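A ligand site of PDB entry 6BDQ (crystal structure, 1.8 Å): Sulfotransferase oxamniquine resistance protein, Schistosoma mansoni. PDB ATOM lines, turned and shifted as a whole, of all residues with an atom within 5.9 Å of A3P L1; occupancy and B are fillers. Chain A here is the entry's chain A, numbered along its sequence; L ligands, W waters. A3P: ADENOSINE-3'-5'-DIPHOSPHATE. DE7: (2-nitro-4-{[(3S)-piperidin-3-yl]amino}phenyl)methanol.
O10 of DE7 L2 lies close to NH1 of Arg 19 (3.4 Å).
OG of Ser 24 sits at hydrogen-bond distance from N7 of A3P L1.
The backbone NH (N) of His 232 is in hydrogen-bond range of an oxygen (O2P) of A3P L1 (3.0 Å).
The guanidinium group of Arg 117 lies within salt-bridge range of an oxygen (O1P) of A3P L1 (2.9 Å).
The backbone NH (N) of Thr 20 lies within hydrogen-bond range of an oxygen (O4P) of A3P L1, at 3.2 Å.
O of Pro 227 is in hydrogen-bond range of N6 of A3P L1, 3.0 Å away.
ND2 of Asn 230 sits at hydrogen-bond distance from O11 of DE7 L2 (3.3 Å).
N of Lys 23 sits at hydrogen-bond distance from O5P of A3P L1, 2.9 Å away.
O4P of A3P L1 is in hydrogen-bond range of N of Thr 22.
The guanidinium group (NH1) of Arg 19 is in salt-bridge range of an oxygen (O6P) of A3P L1 (2.8 Å).
The side-chain hydroxyl (OG1) of Thr 22 lies within hydrogen-bond range of an oxygen (O4P) of A3P L1.
An oxygen (O5') of A3P L1 is in hydrogen-bond range of the backbone NH (N) of Gly 21, 3.0 Å away.
OG of Ser 125 sits at hydrogen-bond distance from O2P of A3P L1.
An oxygen (O4P) of A3P L1 lies within hydrogen-bond range of the backbone NH (N) of Arg 19 (3.0 Å).
O5P of A3P L1 sits at hydrogen-bond distance from ND2 of Asn 230, 3.0 Å away.
OD2 of Asp 93 sits at hydrogen-bond distance from O9 of DE7 L2, at 2.5 Å.
A ring nitrogen (NE2) of His 39 lies within hydrogen-bond range of the side-chain hydroxyl of Thr 22 (3.0 Å).
O of Pro 227 lies within hydrogen-bond range of OG of Ser 24 (3.2 Å).
OG1 of Thr 20 lies within hydrogen-bond range of O of Leu 17 (2.6 Å).
OG of Ser 24 lies within hydrogen-bond range of N of Val 229, 3.1 Å away.
A ring nitrogen (NE2) of His 232 lies close to a ring nitrogen (NE2) of His 233 (3.5 Å).
The backbone carbonyl oxygen of Arg 19 lies within hydrogen-bond range of the guanidinium group of Arg 117, 2.8 Å away.
OG of Ser 125 sits at hydrogen-bond distance from NE of Arg 19, at 2.8 Å.
The backbone carbonyl oxygen of Asn 230 is in hydrogen-bond range of the guanidinium group of Arg 19 (2.8 Å).
Merely in contact with A3P L1: Pro 18 (3.96 Å), Leu 205 (3.5 Å), Gly 206 (3.7 Å), Tyr 226 (3.8 Å), Cys 228 (3.7 Å), Val 229 (3.4 Å) and Ser 231 (3.3 Å).
Within 4 Å of A3P L1: Pro 18, Arg 19, Thr 20, Gly 21, Thr 22, Lys 23, Ser 24, Arg 117, Ser 125, Leu 205, Gly 206, Tyr 226, Pro 227, Cys 228, Val 229, Asn 230, Ser 231 and His 232.
Water W3 lies within hydrogen-bond range of an oxygen (O5P) of A3P L1 (2.7 Å), the backbone NH of Ser 24 (2.8 Å), the backbone carbonyl oxygen of Val 229 (3.0 Å) and the backbone NH of Lys 23 (3.3 Å).
Water W4 bridges an oxygen (O1P) of A3P L1 (2.7 Å) and the backbone carbonyl oxygen (O) of Asp 121 (3.0 Å).
Water W2 lies within hydrogen-bond range of an oxygen (O9) of DE7 L2 (2.7 Å), an oxygen (O6P) of A3P L1 (2.8 Å), the side-chain amide nitrogen of Asn 230 (3.1 Å), a ring nitrogen (NE2) of His 39 (3.1 Å) and the side-chain hydroxyl of Thr 22 (3.4 Å).
Water W6 bridges SG of Cys 228 (3.2 Å) and O2' of A3P L1 (3.3 Å).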
ATOM      1  N   LEU A  17     -35.734 -15.369  16.990  1.00  0.00           N
ATOM      2  CA  LEU A  17     -36.081 -14.040  17.458  1.00  0.00           C
ATOM      3  C   LEU A  17     -34.834 -13.269  17.908  1.00  0.00           C
ATOM      4  O   LEU A  17     -33.781 -13.869  18.174  1.00  0.00           O
ATOM      5  CB  LEU A  17     -37.066 -14.154  18.621  1.00  0.00           C
ATOM      6  CG  LEU A  17     -38.434 -14.689  18.187  1.00  0.00           C
ATOM      7  CD1 LEU A  17     -39.246 -15.131  19.393  1.00  0.00           C
ATOM      8  CD2 LEU A  17     -39.183 -13.656  17.352  1.00  0.00           C
ATOM      9  N   PRO A  18     -34.922 -11.948  17.992  1.00  0.00           N
ATOM     10  CA  PRO A  18     -33.772 -11.182  18.491  1.00  0.00           C
ATOM     11  C   PRO A  18     -33.388 -11.652  19.886  1.00  0.00           C
ATOM     12  O   PRO A  18     -34.243 -12.099  20.655  1.00  0.00           O
ATOM     13  CB  PRO A  18     -34.310  -9.728  18.529  1.00  0.00           C
ATOM     14  CG  PRO A  18     -35.810  -9.870  18.531  1.00  0.00           C
ATOM     15  CD  PRO A  18     -36.066 -11.073  17.663  1.00  0.00           C
ATOM     16  N   ARG A  19     -32.096 -11.562  20.204  1.00  0.00           N
ATOM     17  CA  ARG A  19     -31.541 -12.006  21.486  1.00  0.00           C
ATOM     18  C   ARG A  19     -31.454 -13.524  21.616  1.00  0.00           C
ATOM     19  O   ARG A  19     -31.416 -14.050  22.736  1.00  0.00           O
ATOM     20  CB  ARG A  19     -32.220 -11.360  22.725  1.00  0.00           C
ATOM     21  CG  ARG A  19     -32.436  -9.831  22.581  1.00  0.00           C
ATOM     22  CD  ARG A  19     -31.132  -9.110  22.178  1.00  0.00           C
ATOM     23  NE  ARG A  19     -30.086  -9.273  23.180  1.00  0.00           N
ATOM     24  CZ  ARG A  19     -28.826  -8.863  23.038  1.00  0.00           C
ATOM     25  NH1 ARG A  19     -28.438  -8.278  21.904  1.00  0.00           N
ATOM     26  NH2 ARG A  19     -27.944  -9.036  24.027  1.00  0.00           N
ATOM     27  N   THR A  20     -31.385 -14.234  20.487  1.00  0.00           N
ATOM     28  CA  THR A  20     -31.130 -15.677  20.479  1.00  0.00           C
ATOM     29  C   THR A  20     -29.830 -16.024  19.758  1.00  0.00           C
ATOM     30  O   THR A  20     -29.682 -17.133  19.239  1.00  0.00           O
ATOM     31  CB  THR A  20     -32.294 -16.452  19.872  1.00  0.00           C
ATOM     32  OG1 THR A  20     -32.463 -16.093  18.496  1.00  0.00           O
ATOM     33  CG2 THR A  20     -33.587 -16.178  20.637  1.00  0.00           C
ATOM     34  N   GLY A  21     -28.875 -15.109  19.720  1.00  0.00           N
ATOM     35  CA  GLY A  21     -27.630 -15.358  19.022  1.00  0.00           C
ATOM     36  C   GLY A  21     -27.603 -14.968  17.556  1.00  0.00           C
ATOM     37  O   GLY A  21     -26.807 -15.527  16.785  1.00  0.00           O
ATOM     38  N   THR A  22     -28.447 -14.018  17.133  1.00  0.00           N
ATOM     39  CA  THR A  22     -28.543 -13.703  15.717  1.00  0.00           C
ATOM     40  C   THR A  22     -27.296 -13.002  15.189  1.00  0.00           C
ATOM     41  O   THR A  22     -26.895 -13.239  14.054  1.00  0.00           O
ATOM     42  CB  THR A  22     -29.799 -12.869  15.402  1.00  0.00           C
ATOM     43  OG1 THR A  22     -29.723 -11.630  16.096  1.00  0.00           O
ATOM     44  CG2 THR A  22     -31.076 -13.616  15.788  1.00  0.00           C
ATOM     45  N   LYS A  23     -26.679 -12.117  15.989  1.00  0.00           N
ATOM     46  CA  LYS A  23     -25.504 -11.397  15.468  1.00  0.00           C
ATOM     47  C   LYS A  23     -24.299 -12.330  15.341  1.00  0.00           C
ATOM     48  O   LYS A  23     -23.525 -12.219  14.385  1.00  0.00           O
ATOM     49  CB  LYS A  23     -25.153 -10.183  16.333  1.00  0.00           C
ATOM     50  CG  LYS A  23     -24.003  -9.295  15.758  1.00  0.00           C
ATOM     51  CD  LYS A  23     -24.322  -8.867  14.334  1.00  0.00           C
ATOM     52  CE  LYS A  23     -23.390  -7.771  13.742  1.00  0.00           C
ATOM     53  NZ  LYS A  23     -21.951  -8.126  13.600  1.00  0.00           N
ATOM     54  N   SER A  24     -24.132 -13.237  16.292  1.00  0.00           N
ATOM     55  CA  SER A  24     -23.127 -14.277  16.124  1.00  0.00           C
ATOM     56  C   SER A  24     -23.412 -15.131  14.900  1.00  0.00           C
ATOM     57  O   SER A  24     -22.491 -15.466  14.140  1.00  0.00           O
ATOM     58  CB  SER A  24     -23.038 -15.152  17.387  1.00  0.00           C
ATOM     59  OG  SER A  24     -22.469 -14.433  18.475  1.00  0.00           O
ATOM     60  N   HIS A  39     -29.543  -8.528   8.982  1.00  0.00           N
ATOM     61  CA  HIS A  39     -29.673  -8.412  10.435  1.00  0.00           C
ATOM     62  C   HIS A  39     -30.135  -6.985  10.685  1.00  0.00           C
ATOM     63  O   HIS A  39     -29.979  -6.111   9.825  1.00  0.00           O
ATOM     64  CB  HIS A  39     -28.316  -8.651  11.107  1.00  0.00           C
ATOM     65  CG  HIS A  39     -28.362  -8.719  12.604  1.00  0.00           C
ATOM     66  ND1 HIS A  39     -28.206  -7.609  13.413  1.00  0.00           N
ATOM     67  CD2 HIS A  39     -28.486  -9.769  13.450  1.00  0.00           C
ATOM     68  CE1 HIS A  39     -28.273  -7.969  14.679  1.00  0.00           C
ATOM     69  NE2 HIS A  39     -28.442  -9.275  14.736  1.00  0.00           N
ATOM     70  N   ASP A  93     -32.833 -12.152  12.340  1.00  0.00           N
ATOM     71  CA  ASP A  93     -33.209 -11.043  13.226  1.00  0.00           C
ATOM     72  C   ASP A  93     -34.453 -10.320  12.744  1.00  0.00           C
ATOM     73  O   ASP A  93     -34.935 -10.571  11.630  1.00  0.00           O
ATOM     74  CB  ASP A  93     -32.028 -10.057  13.358  1.00  0.00           C
ATOM     75  CG  ASP A  93     -32.157  -9.080  14.532  1.00  0.00           C
ATOM     76  OD1 ASP A  93     -33.043  -9.244  15.398  1.00  0.00           O
ATOM     77  OD2 ASP A  93     -31.340  -8.145  14.586  1.00  0.00           O
ATOM     78  N   ARG A 117     -33.304 -20.341  23.019  1.00  0.00           N
ATOM     79  CA  ARG A 117     -32.597 -20.365  24.290  1.00  0.00           C
ATOM     80  C   ARG A 117     -33.624 -20.343  25.409  1.00  0.00           C
ATOM     81  O   ARG A 117     -34.831 -20.204  25.173  1.00  0.00           O
ATOM     82  CB  ARG A 117     -31.694 -19.137  24.439  1.00  0.00           C
ATOM     83  CG  ARG A 117     -32.506 -17.844  24.586  1.00  0.00           C
ATOM     84  CD  ARG A 117     -31.641 -16.587  24.585  1.00  0.00           C
ATOM     85  NE  ARG A 117     -30.675 -16.537  25.686  1.00  0.00           N
ATOM     86  CZ  ARG A 117     -29.920 -15.461  25.931  1.00  0.00           C
ATOM     87  NH1 ARG A 117     -30.060 -14.376  25.186  1.00  0.00           N
ATOM     88  NH2 ARG A 117     -29.048 -15.463  26.929  1.00  0.00           N
ATOM     89  N   ASP A 121     -33.926 -16.152  30.215  1.00  0.00           N
ATOM     90  CA  ASP A 121     -32.723 -15.469  29.750  1.00  0.00           C
ATOM     91  C   ASP A 121     -33.016 -14.605  28.536  1.00  0.00           C
ATOM     92  O   ASP A 121     -32.467 -13.503  28.400  1.00  0.00           O
ATOM     93  CB  ASP A 121     -31.662 -16.488  29.354  1.00  0.00           C
ATOM     94  CG  ASP A 121     -31.018 -17.165  30.541  1.00  0.00           C
ATOM     95  OD1 ASP A 121     -31.255 -16.739  31.703  1.00  0.00           O
ATOM     96  OD2 ASP A 121     -30.265 -18.120  30.297  1.00  0.00           O
ATOM     97  N   SER A 125     -32.612 -10.523  28.474  1.00  0.00           N
ATOM     98  CA  SER A 125     -31.755  -9.927  27.466  1.00  0.00           C
ATOM     99  C   SER A 125     -32.522  -8.907  26.629  1.00  0.00           C
ATOM    100  O   SER A 125     -32.020  -7.815  26.335  1.00  0.00           O
ATOM    101  CB  SER A 125     -31.222 -11.054  26.564  1.00  0.00           C
ATOM    102  OG  SER A 125     -30.236 -10.582  25.656  1.00  0.00           O
ATOM    103  N   VAL A 129     -31.853  -4.596  26.140  1.00  0.00           N
ATOM    104  CA  VAL A 129     -31.287  -4.238  24.835  1.00  0.00           C
ATOM    105  C   VAL A 129     -32.340  -3.649  23.898  1.00  0.00           C
ATOM    106  O   VAL A 129     -32.123  -2.606  23.276  1.00  0.00           O
ATOM    107  CB  VAL A 129     -30.555  -5.425  24.188  1.00  0.00           C
ATOM    108  CG1 VAL A 129     -30.035  -5.030  22.803  1.00  0.00           C
ATOM    109  CG2 VAL A 129     -29.410  -5.907  25.086  1.00  0.00           C
ATOM    110  N   LEU A 205     -28.827 -21.856  21.621  1.00  0.00           N
ATOM    111  CA  LEU A 205     -27.742 -20.897  21.807  1.00  0.00           C
ATOM    112  C   LEU A 205     -26.546 -21.590  22.453  1.00  0.00           C
ATOM    113  O   LEU A 205     -26.686 -22.265  23.465  1.00  0.00           O
ATOM    114  CB  LEU A 205     -28.227 -19.777  22.718  1.00  0.00           C
ATOM    115  CG  LEU A 205     -27.377 -18.535  22.853  1.00  0.00           C
ATOM    116  CD1 LEU A 205     -27.055 -17.955  21.495  1.00  0.00           C
ATOM    117  CD2 LEU A 205     -28.158 -17.526  23.684  1.00  0.00           C
ATOM    118  N   GLY A 206     -25.367 -21.421  21.836  1.00  0.00           N
ATOM    119  CA  GLY A 206     -24.135 -22.039  22.300  1.00  0.00           C
ATOM    120  C   GLY A 206     -23.779 -23.365  21.653  1.00  0.00           C
ATOM    121  O   GLY A 206     -22.759 -23.968  22.046  1.00  0.00           O
ATOM    122  N   TYR A 226     -16.348 -20.131  17.007  1.00  0.00           N
ATOM    123  CA  TYR A 226     -17.684 -19.682  16.655  1.00  0.00           C
ATOM    124  C   TYR A 226     -17.924 -18.334  17.314  1.00  0.00           C
ATOM    125  O   TYR A 226     -17.620 -18.173  18.501  1.00  0.00           O
ATOM    126  CB  TYR A 226     -18.739 -20.697  17.104  1.00  0.00           C
ATOM    127  CG  TYR A 226     -20.123 -20.326  16.619  1.00  0.00           C
ATOM    128  CD1 TYR A 226     -20.557 -20.691  15.343  1.00  0.00           C
ATOM    129  CD2 TYR A 226     -20.987 -19.599  17.423  1.00  0.00           C
ATOM    130  CE1 TYR A 226     -21.820 -20.328  14.883  1.00  0.00           C
ATOM    131  CE2 TYR A 226     -22.247 -19.237  16.976  1.00  0.00           C
ATOM    132  CZ  TYR A 226     -22.655 -19.597  15.723  1.00  0.00           C
ATOM    133  OH  TYR A 226     -23.916 -19.217  15.300  1.00  0.00           O
ATOM    134  N   PRO A 227     -18.441 -17.345  16.587  1.00  0.00           N
ATOM    135  CA  PRO A 227     -18.569 -15.997  17.164  1.00  0.00           C
ATOM    136  C   PRO A 227     -19.371 -15.987  18.454  1.00  0.00           C
ATOM    137  O   PRO A 227     -20.325 -16.748  18.651  1.00  0.00           O
ATOM    138  CB  PRO A 227     -19.288 -15.210  16.066  1.00  0.00           C
ATOM    139  CG  PRO A 227     -18.989 -15.952  14.795  1.00  0.00           C
ATOM    140  CD  PRO A 227     -18.851 -17.406  15.180  1.00  0.00           C
ATOM    141  N   CYS A 228     -18.964 -15.088  19.359  1.00  0.00           N
ATOM    142  CA  CYS A 228     -19.666 -14.848  20.617  1.00  0.00           C
ATOM    143  C   CYS A 228     -19.651 -13.334  20.797  1.00  0.00           C
ATOM    144  O   CYS A 228     -18.723 -12.771  21.366  1.00  0.00           O
ATOM    145  CB  CYS A 228     -18.990 -15.569  21.777  1.00  0.00           C
ATOM    146  SG  CYS A 228     -19.990 -15.567  23.277  1.00  0.00           S
ATOM    147  N   VAL A 229     -20.673 -12.665  20.240  1.00  0.00           N
ATOM    148  CA  VAL A 229     -20.758 -11.219  20.267  1.00  0.00           C
ATOM    149  C   VAL A 229     -22.173 -10.823  20.655  1.00  0.00           C
ATOM    150  O   VAL A 229     -23.098 -11.614  20.613  1.00  0.00           O
ATOM    151  CB  VAL A 229     -20.396 -10.579  18.901  1.00  0.00           C
ATOM    152  CG1 VAL A 229     -18.971 -10.930  18.491  1.00  0.00           C
ATOM    153  CG2 VAL A 229     -21.404 -11.030  17.840  1.00  0.00           C
ATOM    154  N   ASN A 230     -22.322  -9.540  21.004  1.00  0.00           N
ATOM    155  CA  ASN A 230     -23.633  -8.926  21.181  1.00  0.00           C
ATOM    156  C   ASN A 230     -24.320  -9.306  22.497  1.00  0.00           C
ATOM    157  O   ASN A 230     -25.559  -9.302  22.577  1.00  0.00           O
ATOM    158  CB  ASN A 230     -24.544  -9.157  19.970  1.00  0.00           C
ATOM    159  CG  ASN A 230     -25.585  -8.059  19.828  1.00  0.00           C
ATOM    160  OD1 ASN A 230     -25.383  -6.961  20.321  1.00  0.00           O
ATOM    161  ND2 ASN A 230     -26.701  -8.362  19.178  1.00  0.00           N
ATOM    162  N   SER A 231     -23.535  -9.589  23.542  1.00  0.00           N
ATOM    163  CA  SER A 231     -24.124  -9.769  24.860  1.00  0.00           C
ATOM    164  C   SER A 231     -24.767  -8.467  25.336  1.00  0.00           C
ATOM    165  O   SER A 231     -24.431  -7.379  24.861  1.00  0.00           O
ATOM    166  CB  SER A 231     -23.051 -10.189  25.871  1.00  0.00           C
ATOM    167  OG  SER A 231     -22.157  -9.103  26.115  1.00  0.00           O
ATOM    168  N   HIS A 232     -25.709  -8.587  26.265  1.00  0.00           N
ATOM    169  CA  HIS A 232     -26.345  -7.353  26.756  1.00  0.00           C
ATOM    170  C   HIS A 232     -25.318  -6.446  27.419  1.00  0.00           C
ATOM    171  O   HIS A 232     -25.444  -5.211  27.352  1.00  0.00           O
ATOM    172  CB  HIS A 232     -27.545  -7.649  27.656  1.00  0.00           C
ATOM    173  CG  HIS A 232     -27.190  -8.260  28.982  1.00  0.00           C
ATOM    174  ND1 HIS A 232     -26.814  -7.502  30.069  1.00  0.00           N
ATOM    175  CD2 HIS A 232     -27.197  -9.544  29.407  1.00  0.00           C
ATOM    176  CE1 HIS A 232     -26.561  -8.301  31.093  1.00  0.00           C
ATOM    177  NE2 HIS A 232     -26.809  -9.543  30.720  1.00  0.00           N
ATOM    178  N   HIS A 233     -24.281  -7.030  28.037  1.00  0.00           N
ATOM    179  CA  HIS A 233     -23.205  -6.220  28.613  1.00  0.00           C
ATOM    180  C   HIS A 233     -22.498  -5.391  27.548  1.00  0.00           C
ATOM    181  O   HIS A 233     -22.168  -4.225  27.780  1.00  0.00           O
ATOM    182  CB  HIS A 233     -22.186  -7.122  29.322  1.00  0.00           C
ATOM    183  CG  HIS A 233     -22.753  -7.940  30.436  1.00  0.00           C
ATOM    184  ND1 HIS A 233     -23.077  -7.413  31.668  1.00  0.00           N
ATOM    185  CD2 HIS A 233     -23.004  -9.272  30.522  1.00  0.00           C
ATOM    186  CE1 HIS A 233     -23.526  -8.376  32.458  1.00  0.00           C
ATOM    187  NE2 HIS A 233     -23.491  -9.520  31.784  1.00  0.00           N
HETATM  188  P1  A3P L   1     -27.174 -12.050  26.625  1.00  0.00           P
HETATM  189  O1P A3P L   1     -27.943 -12.909  27.573  1.00  0.00           O
HETATM  190  O2P A3P L   1     -27.816 -10.706  26.389  1.00  0.00           O
HETATM  191  O3P A3P L   1     -25.691 -11.952  26.882  1.00  0.00           O
HETATM  192  P2  A3P L   1     -28.673 -11.373  19.371  1.00  0.00           P
HETATM  193  O4P A3P L   1     -29.671 -12.240  18.666  1.00  0.00           O
HETATM  194  O5P A3P L   1     -27.330 -11.218  18.684  1.00  0.00           O
HETATM  195  O6P A3P L   1     -29.190 -10.087  19.928  1.00  0.00           O
HETATM  196  O5' A3P L   1     -28.364 -12.324  20.639  1.00  0.00           O
HETATM  197  C5' A3P L   1     -27.402 -11.945  21.627  1.00  0.00           C
HETATM  198  C4' A3P L   1     -27.485 -12.893  22.837  1.00  0.00           C
HETATM  199  O4' A3P L   1     -26.927 -14.153  22.477  1.00  0.00           O
HETATM  200  C3' A3P L   1     -26.657 -12.405  24.025  1.00  0.00           C
HETATM  201  O3' A3P L   1     -27.267 -12.883  25.231  1.00  0.00           O
HETATM  202  C2' A3P L   1     -25.322 -13.080  23.807  1.00  0.00           C
HETATM  203  O2' A3P L   1     -24.545 -13.183  25.016  1.00  0.00           O
HETATM  204  C1' A3P L   1     -25.793 -14.429  23.305  1.00  0.00           C
HETATM  205  N9  A3P L   1     -24.788 -15.116  22.465  1.00  0.00           N
HETATM  206  C8  A3P L   1     -24.303 -14.700  21.276  1.00  0.00           C
HETATM  207  N7  A3P L   1     -23.391 -15.595  20.792  1.00  0.00           N
HETATM  208  C5  A3P L   1     -23.320 -16.602  21.689  1.00  0.00           C
HETATM  209  C6  A3P L   1     -22.566 -17.856  21.811  1.00  0.00           C
HETATM  210  N6  A3P L   1     -21.702 -18.212  20.838  1.00  0.00           N
HETATM  211  N1  A3P L   1     -22.760 -18.619  22.913  1.00  0.00           N
HETATM  212  C2  A3P L   1     -23.632 -18.243  23.883  1.00  0.00           C
HETATM  213  N3  A3P L   1     -24.360 -17.110  23.854  1.00  0.00           N
HETATM  214  C4  A3P L   1     -24.240 -16.267  22.802  1.00  0.00           C
HETATM  215  C1  DE7 L   2     -32.803  -3.909  17.758  1.00  0.00           C
HETATM  216  C15 DE7 L   2     -29.677  -0.907  19.926  1.00  0.00           C
HETATM  217  C16 DE7 L   2     -28.980  -0.673  18.597  1.00  0.00           C
HETATM  218  C17 DE7 L   2     -27.635   0.024  18.755  1.00  0.00           C
HETATM  219  C18 DE7 L   2     -27.783   1.294  19.567  1.00  0.00           C
HETATM  220  C2  DE7 L   2     -32.032  -5.030  18.019  1.00  0.00           C
HETATM  221  C20 DE7 L   2     -29.713   0.404  20.724  1.00  0.00           C
HETATM  222  C3  DE7 L   2     -30.896  -4.924  18.832  1.00  0.00           C
HETATM  223  C4  DE7 L   2     -30.567  -3.686  19.388  1.00  0.00           C
HETATM  224  C5  DE7 L   2     -31.333  -2.554  19.119  1.00  0.00           C
HETATM  225  C6  DE7 L   2     -32.464  -2.673  18.303  1.00  0.00           C
HETATM  226  C7  DE7 L   2     -32.482  -6.325  17.375  1.00  0.00           C
HETATM  227  N12 DE7 L   2     -31.030  -1.345  19.658  1.00  0.00           N
HETATM  228  N19 DE7 L   2     -28.349   0.941  20.880  1.00  0.00           N
HETATM  229  N8  DE7 L   2     -30.071  -6.018  19.176  1.00  0.00           N
HETATM  230  O10 DE7 L   2     -30.559  -7.096  19.547  1.00  0.00           O
HETATM  231  O11 DE7 L   2     -28.835  -5.907  19.172  1.00  0.00           O
HETATM  232  O9  DE7 L   2     -31.344  -6.934  16.746  1.00  0.00           O
HETATM  233  O   HOH W   1     -24.228 -12.097  29.072  1.00  0.00           O
HETATM  234  O   HOH W   2     -29.311  -8.557  17.597  1.00  0.00           O
HETATM  235  O   HOH W   3     -25.178 -12.805  18.885  1.00  0.00           O
HETATM  236  O   HOH W   4     -29.806 -12.880  29.543  1.00  0.00           O
HETATM  237  O   HOH W   5     -20.413 -20.960  20.714  1.00  0.00           O
HETATM  238  O   HOH W   6     -21.237 -13.484  25.320  1.00  0.00           O
HETATM  239  O   HOH W   7     -25.458 -16.832  26.915  1.00  0.00           O
